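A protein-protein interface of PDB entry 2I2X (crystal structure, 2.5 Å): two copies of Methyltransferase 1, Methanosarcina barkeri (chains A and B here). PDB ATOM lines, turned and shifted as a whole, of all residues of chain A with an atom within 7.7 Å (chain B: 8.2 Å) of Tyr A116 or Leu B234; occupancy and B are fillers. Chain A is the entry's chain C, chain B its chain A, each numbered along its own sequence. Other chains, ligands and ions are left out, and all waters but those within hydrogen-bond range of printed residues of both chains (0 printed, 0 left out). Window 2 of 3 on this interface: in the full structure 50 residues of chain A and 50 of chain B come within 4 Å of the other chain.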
ATOM      1  N   MET A  70      -8.920  -8.255   6.982  1.00  0.00           N
ATOM      2  CA  MET A  70      -9.204  -6.974   6.308  1.00  0.00           C
ATOM      3  C   MET A  70     -10.667  -6.587   6.511  1.00  0.00           C
ATOM      4  O   MET A  70     -10.988  -5.407   6.708  1.00  0.00           O
ATOM      5  CB  MET A  70      -8.934  -7.028   4.794  1.00  0.00           C
ATOM      6  CG  MET A  70      -7.520  -7.504   4.351  1.00  0.00           C
ATOM      7  SD  MET A  70      -6.117  -6.594   5.054  1.00  0.00           S
ATOM      8  CE  MET A  70      -6.333  -4.943   4.386  1.00  0.00           C
ATOM      9  N   GLU A  71     -11.568  -7.561   6.481  1.00  0.00           N
ATOM     10  CA  GLU A  71     -12.954  -7.216   6.716  1.00  0.00           C
ATOM     11  C   GLU A  71     -13.088  -6.555   8.090  1.00  0.00           C
ATOM     12  O   GLU A  71     -13.736  -5.518   8.224  1.00  0.00           O
ATOM     13  CB  GLU A  71     -13.885  -8.426   6.553  1.00  0.00           C
ATOM     14  CG  GLU A  71     -15.402  -8.132   6.668  1.00  0.00           C
ATOM     15  CD  GLU A  71     -16.003  -7.193   5.579  1.00  0.00           C
ATOM     16  OE1 GLU A  71     -15.335  -6.855   4.563  1.00  0.00           O
ATOM     17  OE2 GLU A  71     -17.185  -6.798   5.758  1.00  0.00           O
ATOM     18  N   ARG A  72     -12.439  -7.133   9.096  1.00  0.00           N
ATOM     19  CA  ARG A  72     -12.621  -6.680  10.464  1.00  0.00           C
ATOM     20  C   ARG A  72     -12.062  -5.277  10.672  1.00  0.00           C
ATOM     21  O   ARG A  72     -12.684  -4.441  11.347  1.00  0.00           O
ATOM     22  CB  ARG A  72     -11.959  -7.645  11.443  1.00  0.00           C
ATOM     23  CG  ARG A  72     -12.259  -7.246  12.839  1.00  0.00           C
ATOM     24  CD  ARG A  72     -13.799  -7.276  13.060  1.00  0.00           C
ATOM     25  NE  ARG A  72     -13.988  -7.853  14.368  1.00  0.00           N
ATOM     26  CZ  ARG A  72     -14.582  -8.994  14.636  1.00  0.00           C
ATOM     27  NH1 ARG A  72     -15.190  -9.681  13.707  1.00  0.00           N
ATOM     28  NH2 ARG A  72     -14.606  -9.403  15.885  1.00  0.00           N
ATOM     29  N   MET A  73     -10.880  -5.042  10.083  1.00  0.00           N
ATOM     30  CA  MET A  73     -10.209  -3.766  10.159  1.00  0.00           C
ATOM     31  C   MET A  73     -11.115  -2.650   9.622  1.00  0.00           C
ATOM     32  O   MET A  73     -11.279  -1.608  10.260  1.00  0.00           O
ATOM     33  CB  MET A  73      -8.854  -3.815   9.391  1.00  0.00           C
ATOM     34  CG  MET A  73      -7.722  -4.688   9.996  1.00  0.00           C
ATOM     35  SD  MET A  73      -7.569  -4.660  11.816  1.00  0.00           S
ATOM     36  CE  MET A  73      -6.502  -3.299  11.959  1.00  0.00           C
ATOM     37  N   VAL A  74     -11.719  -2.847   8.459  1.00  0.00           N
ATOM     38  CA  VAL A  74     -12.536  -1.772   7.913  1.00  0.00           C
ATOM     39  C   VAL A  74     -13.874  -1.662   8.659  1.00  0.00           C
ATOM     40  O   VAL A  74     -14.440  -0.573   8.743  1.00  0.00           O
ATOM     41  CB  VAL A  74     -12.693  -1.823   6.361  1.00  0.00           C
ATOM     42  CG1 VAL A  74     -11.314  -1.638   5.652  1.00  0.00           C
ATOM     43  CG2 VAL A  74     -13.355  -3.115   5.899  1.00  0.00           C
ATOM     44  N   GLN A  75     -14.361  -2.745   9.263  1.00  0.00           N
ATOM     45  CA  GLN A  75     -15.610  -2.620   9.994  1.00  0.00           C
ATOM     46  C   GLN A  75     -15.456  -1.848  11.299  1.00  0.00           C
ATOM     47  O   GLN A  75     -16.437  -1.319  11.828  1.00  0.00           O
ATOM     48  CB  GLN A  75     -16.251  -3.973  10.265  1.00  0.00           C
ATOM     49  CG  GLN A  75     -16.749  -4.681   9.043  1.00  0.00           C
ATOM     50  CD  GLN A  75     -18.119  -4.224   8.600  1.00  0.00           C
ATOM     51  OE1 GLN A  75     -18.703  -3.263   9.104  1.00  0.00           O
ATOM     52  NE2 GLN A  75     -18.629  -4.909   7.629  1.00  0.00           N
ATOM     53  N   VAL A  76     -14.240  -1.797  11.843  1.00  0.00           N
ATOM     54  CA  VAL A  76     -14.030  -1.113  13.136  1.00  0.00           C
ATOM     55  C   VAL A  76     -13.227   0.191  12.939  1.00  0.00           C
ATOM     56  O   VAL A  76     -12.967   0.947  13.864  1.00  0.00           O
ATOM     57  CB  VAL A  76     -13.450  -2.069  14.199  1.00  0.00           C
ATOM     58  CG1 VAL A  76     -13.483  -1.444  15.595  1.00  0.00           C
ATOM     59  CG2 VAL A  76     -14.235  -3.333  14.206  1.00  0.00           C
ATOM     60  N   GLY A  77     -12.869   0.489  11.712  1.00  0.00           N
ATOM     61  CA  GLY A  77     -12.352   1.822  11.452  1.00  0.00           C
ATOM     62  C   GLY A  77     -10.841   1.940  11.635  1.00  0.00           C
ATOM     63  O   GLY A  77     -10.336   3.037  11.812  1.00  0.00           O
ATOM     64  N   PHE A  78     -10.122   0.825  11.622  1.00  0.00           N
ATOM     65  CA  PHE A  78      -8.675   0.901  11.818  1.00  0.00           C
ATOM     66  C   PHE A  78      -7.935   1.333  10.553  1.00  0.00           C
ATOM     67  O   PHE A  78      -8.220   0.833   9.475  1.00  0.00           O
ATOM     68  CB  PHE A  78      -8.140  -0.416  12.347  1.00  0.00           C
ATOM     69  CG  PHE A  78      -8.741  -0.816  13.667  1.00  0.00           C
ATOM     70  CD1 PHE A  78      -8.596  -0.002  14.789  1.00  0.00           C
ATOM     71  CD2 PHE A  78      -9.447  -2.005  13.797  1.00  0.00           C
ATOM     72  CE1 PHE A  78      -9.121  -0.387  16.018  1.00  0.00           C
ATOM     73  CE2 PHE A  78      -9.981  -2.401  15.029  1.00  0.00           C
ATOM     74  CZ  PHE A  78      -9.817  -1.584  16.142  1.00  0.00           C
ATOM     75  N   PRO A  79      -6.987   2.275  10.677  1.00  0.00           N
ATOM     76  CA  PRO A  79      -6.297   2.781   9.467  1.00  0.00           C
ATOM     77  C   PRO A  79      -5.240   1.863   8.850  1.00  0.00           C
ATOM     78  O   PRO A  79      -4.869   2.056   7.680  1.00  0.00           O
ATOM     79  CB  PRO A  79      -5.634   4.059   9.942  1.00  0.00           C
ATOM     80  CG  PRO A  79      -5.500   3.916  11.453  1.00  0.00           C
ATOM     81  CD  PRO A  79      -6.512   2.905  11.923  1.00  0.00           C
ATOM     82  N   GLU A 110      -4.915  -6.014  -1.854  1.00  0.00           N
ATOM     83  CA  GLU A 110      -4.962  -4.954  -2.885  1.00  0.00           C
ATOM     84  C   GLU A 110      -6.384  -4.492  -3.136  1.00  0.00           C
ATOM     85  O   GLU A 110      -6.617  -3.308  -3.343  1.00  0.00           O
ATOM     86  CB  GLU A 110      -4.357  -5.409  -4.210  1.00  0.00           C
ATOM     87  CG  GLU A 110      -2.853  -5.409  -4.206  1.00  0.00           C
ATOM     88  CD  GLU A 110      -2.241  -6.180  -5.363  1.00  0.00           C
ATOM     89  OE1 GLU A 110      -2.979  -6.827  -6.147  1.00  0.00           O
ATOM     90  OE2 GLU A 110      -1.000  -6.134  -5.492  1.00  0.00           O
ATOM     91  N   LYS A 111      -7.308  -5.442  -3.113  1.00  0.00           N
ATOM     92  CA  LYS A 111      -8.740  -5.195  -3.279  1.00  0.00           C
ATOM     93  C   LYS A 111      -9.258  -4.285  -2.165  1.00  0.00           C
ATOM     94  O   LYS A 111      -9.847  -3.241  -2.461  1.00  0.00           O
ATOM     95  CB  LYS A 111      -9.511  -6.531  -3.347  1.00  0.00           C
ATOM     96  CG  LYS A 111     -10.998  -6.435  -3.636  1.00  0.00           C
ATOM     97  CD  LYS A 111     -11.788  -7.524  -2.832  1.00  0.00           C
ATOM     98  CE  LYS A 111     -13.333  -7.298  -2.818  1.00  0.00           C
ATOM     99  NZ  LYS A 111     -13.827  -6.636  -1.537  1.00  0.00           N
ATOM    100  N   TYR A 112      -8.998  -4.639  -0.901  1.00  0.00           N
ATOM    101  CA  TYR A 112      -9.388  -3.784   0.225  1.00  0.00           C
ATOM    102  C   TYR A 112      -8.637  -2.439   0.237  1.00  0.00           C
ATOM    103  O   TYR A 112      -9.187  -1.416   0.664  1.00  0.00           O
ATOM    104  CB  TYR A 112      -9.194  -4.494   1.565  1.00  0.00           C
ATOM    105  CG  TYR A 112     -10.280  -5.458   1.935  1.00  0.00           C
ATOM    106  CD1 TYR A 112     -10.255  -6.771   1.470  1.00  0.00           C
ATOM    107  CD2 TYR A 112     -11.320  -5.072   2.791  1.00  0.00           C
ATOM    108  CE1 TYR A 112     -11.251  -7.682   1.813  1.00  0.00           C
ATOM    109  CE2 TYR A 112     -12.329  -5.964   3.137  1.00  0.00           C
ATOM    110  CZ  TYR A 112     -12.294  -7.268   2.643  1.00  0.00           C
ATOM    111  OH  TYR A 112     -13.278  -8.168   2.996  1.00  0.00           O
ATOM    112  N   HIS A 113      -7.385  -2.423  -0.206  1.00  0.00           N
ATOM    113  CA  HIS A 113      -6.681  -1.157  -0.282  1.00  0.00           C
ATOM    114  C   HIS A 113      -7.317  -0.230  -1.330  1.00  0.00           C
ATOM    115  O   HIS A 113      -7.483   0.960  -1.075  1.00  0.00           O
ATOM    116  CB  HIS A 113      -5.189  -1.346  -0.553  1.00  0.00           C
ATOM    117  CG  HIS A 113      -4.419  -0.059  -0.630  1.00  0.00           C
ATOM    118  ND1 HIS A 113      -3.948   0.456  -1.822  1.00  0.00           N
ATOM    119  CD2 HIS A 113      -4.054   0.825   0.330  1.00  0.00           C
ATOM    120  CE1 HIS A 113      -3.312   1.594  -1.591  1.00  0.00           C
ATOM    121  NE2 HIS A 113      -3.355   1.836  -0.293  1.00  0.00           N
ATOM    122  N   ASP A 114      -7.692  -0.779  -2.483  1.00  0.00           N
ATOM    123  CA  ASP A 114      -8.360   0.005  -3.523  1.00  0.00           C
ATOM    124  C   ASP A 114      -9.728   0.496  -3.099  1.00  0.00           C
ATOM    125  O   ASP A 114     -10.085   1.579  -3.445  1.00  0.00           O
ATOM    126  CB  ASP A 114      -8.444  -0.759  -4.849  1.00  0.00           C
ATOM    127  CG  ASP A 114      -7.070  -1.102  -5.407  1.00  0.00           C
ATOM    128  OD1 ASP A 114      -6.080  -0.420  -5.072  1.00  0.00           O
ATOM    129  OD2 ASP A 114      -6.957  -2.071  -6.164  1.00  0.00           O
ATOM    130  N   GLU A 115     -10.487  -0.286  -2.339  1.00  0.00           N
ATOM    131  CA  GLU A 115     -11.844   0.124  -1.967  1.00  0.00           C
ATOM    132  C   GLU A 115     -11.836   1.169  -0.877  1.00  0.00           C
ATOM    133  O   GLU A 115     -12.554   2.148  -0.967  1.00  0.00           O
ATOM    134  CB  GLU A 115     -12.652  -1.042  -1.409  1.00  0.00           C
ATOM    135  CG  GLU A 115     -13.257  -1.955  -2.413  1.00  0.00           C
ATOM    136  CD  GLU A 115     -14.657  -2.392  -1.999  1.00  0.00           C
ATOM    137  OE1 GLU A 115     -15.541  -1.493  -1.868  1.00  0.00           O
ATOM    138  OE2 GLU A 115     -14.860  -3.626  -1.829  1.00  0.00           O
ATOM    139  N   TYR A 116     -11.035   0.931   0.168  1.00  0.00           N
ATOM    140  CA  TYR A 116     -11.131   1.691   1.407  1.00  0.00           C
ATOM    141  C   TYR A 116      -9.967   2.600   1.694  1.00  0.00           C
ATOM    142  O   TYR A 116     -10.112   3.535   2.482  1.00  0.00           O
ATOM    143  CB  TYR A 116     -11.285   0.742   2.570  1.00  0.00           C
ATOM    144  CG  TYR A 116     -12.460  -0.170   2.440  1.00  0.00           C
ATOM    145  CD1 TYR A 116     -13.773   0.303   2.656  1.00  0.00           C
ATOM    146  CD2 TYR A 116     -12.277  -1.496   2.101  1.00  0.00           C
ATOM    147  CE1 TYR A 116     -14.881  -0.552   2.547  1.00  0.00           C
ATOM    148  CE2 TYR A 116     -13.353  -2.360   1.981  1.00  0.00           C
ATOM    149  CZ  TYR A 116     -14.662  -1.884   2.213  1.00  0.00           C
ATOM    150  OH  TYR A 116     -15.709  -2.754   2.086  1.00  0.00           O
ATOM    151  N   GLY A 117      -8.814   2.327   1.079  1.00  0.00           N
ATOM    152  CA  GLY A 117      -7.607   3.119   1.307  1.00  0.00           C
ATOM    153  C   GLY A 117      -6.885   2.725   2.582  1.00  0.00           C
ATOM    154  O   GLY A 117      -6.030   3.489   3.074  1.00  0.00           O
ATOM    155  N   ILE A 118      -7.236   1.548   3.125  1.00  0.00           N
ATOM    156  CA  ILE A 118      -6.614   1.011   4.322  1.00  0.00           C
ATOM    157  C   ILE A 118      -5.141   0.647   4.028  1.00  0.00           C
ATOM    158  O   ILE A 118      -4.844  -0.030   3.047  1.00  0.00           O
ATOM    159  CB  ILE A 118      -7.418  -0.209   4.908  1.00  0.00           C
ATOM    160  CG1 ILE A 118      -6.768  -0.723   6.203  1.00  0.00           C
ATOM    161  CG2 ILE A 118      -7.561  -1.340   3.894  1.00  0.00           C
ATOM    162  CD1 ILE A 118      -7.400  -1.954   6.822  1.00  0.00           C
ATOM    163  N   LYS A 119      -4.233   1.113   4.880  1.00  0.00           N
ATOM    164  CA  LYS A 119      -2.800   0.925   4.701  1.00  0.00           C
ATOM    165  C   LYS A 119      -2.406  -0.485   5.166  1.00  0.00           C
ATOM    166  O   LYS A 119      -2.813  -0.922   6.244  1.00  0.00           O
ATOM    167  CB  LYS A 119      -2.038   1.976   5.508  1.00  0.00           C
ATOM    168  CG  LYS A 119      -2.052   3.397   4.949  1.00  0.00           C
ATOM    169  CD  LYS A 119      -1.993   4.371   6.138  1.00  0.00           C
ATOM    170  CE  LYS A 119      -1.472   5.793   5.813  1.00  0.00           C
ATOM    171  NZ  LYS A 119      -1.695   6.186   4.392  1.00  0.00           N
ATOM    172  N   GLY B 230     -26.742  -3.284  14.779  1.00  0.00           N
ATOM    173  CA  GLY B 230     -26.056  -2.131  14.171  1.00  0.00           C
ATOM    174  C   GLY B 230     -24.724  -2.550  13.552  1.00  0.00           C
ATOM    175  O   GLY B 230     -24.337  -2.076  12.457  1.00  0.00           O
ATOM    176  N   GLY B 231     -24.020  -3.434  14.262  1.00  0.00           N
ATOM    177  CA  GLY B 231     -22.827  -4.103  13.733  1.00  0.00           C
ATOM    178  C   GLY B 231     -21.693  -3.161  13.428  1.00  0.00           C
ATOM    179  O   GLY B 231     -21.530  -2.145  14.091  1.00  0.00           O
ATOM    180  N   GLY B 232     -20.900  -3.488  12.423  1.00  0.00           N
ATOM    181  CA  GLY B 232     -19.749  -2.653  12.064  1.00  0.00           C
ATOM    182  C   GLY B 232     -20.123  -1.369  11.341  1.00  0.00           C
ATOM    183  O   GLY B 232     -21.260  -1.186  10.931  1.00  0.00           O
ATOM    184  N   LEU B 233     -19.161  -0.475  11.184  1.00  0.00           N
ATOM    185  CA  LEU B 233     -19.362   0.759  10.427  1.00  0.00           C
ATOM    186  C   LEU B 233     -20.005   0.606   9.051  1.00  0.00           C
ATOM    187  O   LEU B 233     -20.605   1.544   8.580  1.00  0.00           O
ATOM    188  CB  LEU B 233     -18.028   1.468  10.233  1.00  0.00           C
ATOM    189  CG  LEU B 233     -17.485   2.471  11.257  1.00  0.00           C
ATOM    190  CD1 LEU B 233     -18.123   2.389  12.665  1.00  0.00           C
ATOM    191  CD2 LEU B 233     -15.971   2.277  11.290  1.00  0.00           C
ATOM    192  N   LEU B 234     -19.826  -0.549   8.401  1.00  0.00           N
ATOM    193  CA  LEU B 234     -20.257  -0.763   7.003  1.00  0.00           C
ATOM    194  C   LEU B 234     -21.538  -1.581   6.899  1.00  0.00           C
ATOM    195  O   LEU B 234     -22.032  -1.817   5.798  1.00  0.00           O
ATOM    196  CB  LEU B 234     -19.179  -1.483   6.195  1.00  0.00           C
ATOM    197  CG  LEU B 234     -17.776  -0.865   6.118  1.00  0.00           C
ATOM    198  CD1 LEU B 234     -16.840  -1.926   5.602  1.00  0.00           C
ATOM    199  CD2 LEU B 234     -17.714   0.332   5.242  1.00  0.00           C
ATOM    200  N   ASN B 235     -22.064  -2.020   8.041  1.00  0.00           N
ATOM    201  CA  ASN B 235     -23.329  -2.704   8.071  1.00  0.00           C
ATOM    202  C   ASN B 235     -24.500  -1.809   7.621  1.00  0.00           C
ATOM    203  O   ASN B 235     -24.412  -0.564   7.596  1.00  0.00           O
ATOM    204  CB  ASN B 235     -23.597  -3.256   9.466  1.00  0.00           C
ATOM    205  CG  ASN B 235     -22.931  -4.592   9.709  1.00  0.00           C
ATOM    206  OD1 ASN B 235     -21.739  -4.787   9.466  1.00  0.00           O
ATOM    207  ND2 ASN B 235     -23.710  -5.531  10.193  1.00  0.00           N
ATOM    208  N   LYS B 236     -25.599  -2.458   7.267  1.00  0.00           N
ATOM    209  CA  LYS B 236     -26.771  -1.756   6.826  1.00  0.00           C
ATOM    210  C   LYS B 236     -28.017  -2.294   7.547  1.00  0.00           C
ATOM    211  O   LYS B 236     -29.094  -2.297   6.996  1.00  0.00           O
ATOM    212  CB  LYS B 236     -26.893  -1.871   5.306  1.00  0.00           C
ATOM    213  CG  LYS B 236     -26.813  -3.305   4.777  1.00  0.00           C
ATOM    214  CD  LYS B 236     -26.731  -3.336   3.254  1.00  0.00           C
ATOM    215  CE  LYS B 236     -26.870  -4.756   2.731  1.00  0.00           C
ATOM    216  NZ  LYS B 236     -26.316  -4.873   1.349  1.00  0.00           N
ATOM    217  N   ASN B 237     -27.870  -2.746   8.787  1.00  0.00           N
ATOM    218  CA  ASN B 237     -29.021  -3.309   9.475  1.00  0.00           C
ATOM    219  C   ASN B 237     -29.718  -2.420  10.512  1.00  0.00           C
ATOM    220  O   ASN B 237     -30.882  -2.647  10.842  1.00  0.00           O
ATOM    221  CB  ASN B 237     -28.702  -4.699  10.015  1.00  0.00           C
ATOM    222  CG  ASN B 237     -28.524  -5.736   8.893  1.00  0.00           C
ATOM    223  OD1 ASN B 237     -29.120  -5.623   7.803  1.00  0.00           O
ATOM    224  ND2 ASN B 237     -27.693  -6.742   9.151  1.00  0.00           N
ATOM    225  N   HIS B 240     -26.454   3.599  13.299  1.00  0.00           N
ATOM    226  CA  HIS B 240     -25.754   3.696  14.541  1.00  0.00           C
ATOM    227  C   HIS B 240     -26.317   4.807  15.404  1.00  0.00           C
ATOM    228  O   HIS B 240     -26.312   4.704  16.650  1.00  0.00           O
ATOM    229  CB  HIS B 240     -24.256   3.790  14.276  1.00  0.00           C
ATOM    230  CG  HIS B 240     -23.661   2.491  13.802  1.00  0.00           C
ATOM    231  ND1 HIS B 240     -22.305   2.223  13.847  1.00  0.00           N
ATOM    232  CD2 HIS B 240     -24.243   1.380  13.288  1.00  0.00           C
ATOM    233  CE1 HIS B 240     -22.082   1.007  13.374  1.00  0.00           C
ATOM    234  NE2 HIS B 240     -23.239   0.479  13.021  1.00  0.00           N
ATOM    235  N   ASP B 364     -17.540   6.455  16.377  1.00  0.00           N
ATOM    236  CA  ASP B 364     -18.957   6.135  16.142  1.00  0.00           C
ATOM    237  C   ASP B 364     -19.827   6.927  17.118  1.00  0.00           C
ATOM    238  O   ASP B 364     -19.377   7.238  18.220  1.00  0.00           O
ATOM    239  CB  ASP B 364     -19.194   4.656  16.403  1.00  0.00           C
ATOM    240  CG  ASP B 364     -20.456   4.126  15.749  1.00  0.00           C
ATOM    241  OD1 ASP B 364     -21.472   4.014  16.469  1.00  0.00           O
ATOM    242  OD2 ASP B 364     -20.448   3.825  14.522  1.00  0.00           O
ATOM    243  N   GLU B 418     -26.940   8.396   8.599  1.00  0.00           N
ATOM    244  CA  GLU B 418     -26.919   8.451  10.054  1.00  0.00           C
ATOM    245  C   GLU B 418     -27.556   9.724  10.558  1.00  0.00           C
ATOM    246  O   GLU B 418     -28.207   9.714  11.595  1.00  0.00           O
ATOM    247  CB  GLU B 418     -25.489   8.352  10.587  1.00  0.00           C
ATOM    248  CG  GLU B 418     -25.032   6.937  10.666  1.00  0.00           C
ATOM    249  CD  GLU B 418     -23.532   6.750  10.770  1.00  0.00           C
ATOM    250  OE1 GLU B 418     -22.754   7.663  10.400  1.00  0.00           O
ATOM    251  OE2 GLU B 418     -23.139   5.657  11.224  1.00  0.00           O
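O of Gln A75 is in hydrogen-bond range of N of Leu B233 (2.9 Å). OE1 of Gln A75 sits at hydrogen-bond distance from N of Leu B234 (3.0 Å). OD1 of Asn B235 sits close to OE1 of Gln A75, at 3.4 Å.
The side-chain carboxylate (OE2) of Glu A71 sits at hydrogen-bond distance from the side-chain amide nitrogen (NE2) of Gln A75, 3.0 Å away. The backbone NH (N) of Gly B232 is in hydrogen-bond range of the side-chain amide oxygen (OD1) of Asn B235 (3.3 Å). The backbone carbonyl oxygen (O) of Gly B232 lies within hydrogen-bond range of a ring nitrogen (NE2) of His B240 (3.3 Å).
CD1 of Leu B234 touches CG2 of Val A74, at 3.7 Å. Gly B232 touches Gln A75. Leu B233 touches Val A76. Gly A77 touches Leu B233 (N to CD2, 3.6 Å). Leu B234 touches Tyr A116 (CD1 to OH, 3.8 Å).
Of the printed residues of chain B, Val A76 touches Leu B233. Of chain B, only Leu B234 (3.8 Å) comes within 4 Å of Tyr A116. No residue of chain B comes within 4 Å of Gly A117. Of the printed residues of chain A, Gly B232 touches Gln A75. Of the printed residues of chain A, Leu B233 touches Gln A75 (2.9 Å), Val A76 (3.8 Å) and Gly A77 (3.6 Å). Of chain A, only Val A74 (3.7 Å), Gln A75 (3.0 Å) and Tyr A116 (3.8 Å) come within 4 Å of Leu B234. The nearest residue of chain A that does not touch Leu B234 is Glu A71 (4.9 Å). The nearest printed residue of chain B that does not touch Val A74 is Leu B233 (4.1 Å).
Of the 11 printed residues of chain B, 4 touch a printed residue of chain A. Of the 20 printed residues of chain A, 5 touch a printed residue of chain B. Along chain A the printed residues that touch a printed residue of chain B span positions 74 to 116. Among the printed residues, 8 pairs touch across the chains. Among the printed residues, no Asp or Glu carboxylate lies within 4 Å of a Lys or Arg side-chain nitrogen of the other chain.
No position is printed for both chains.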
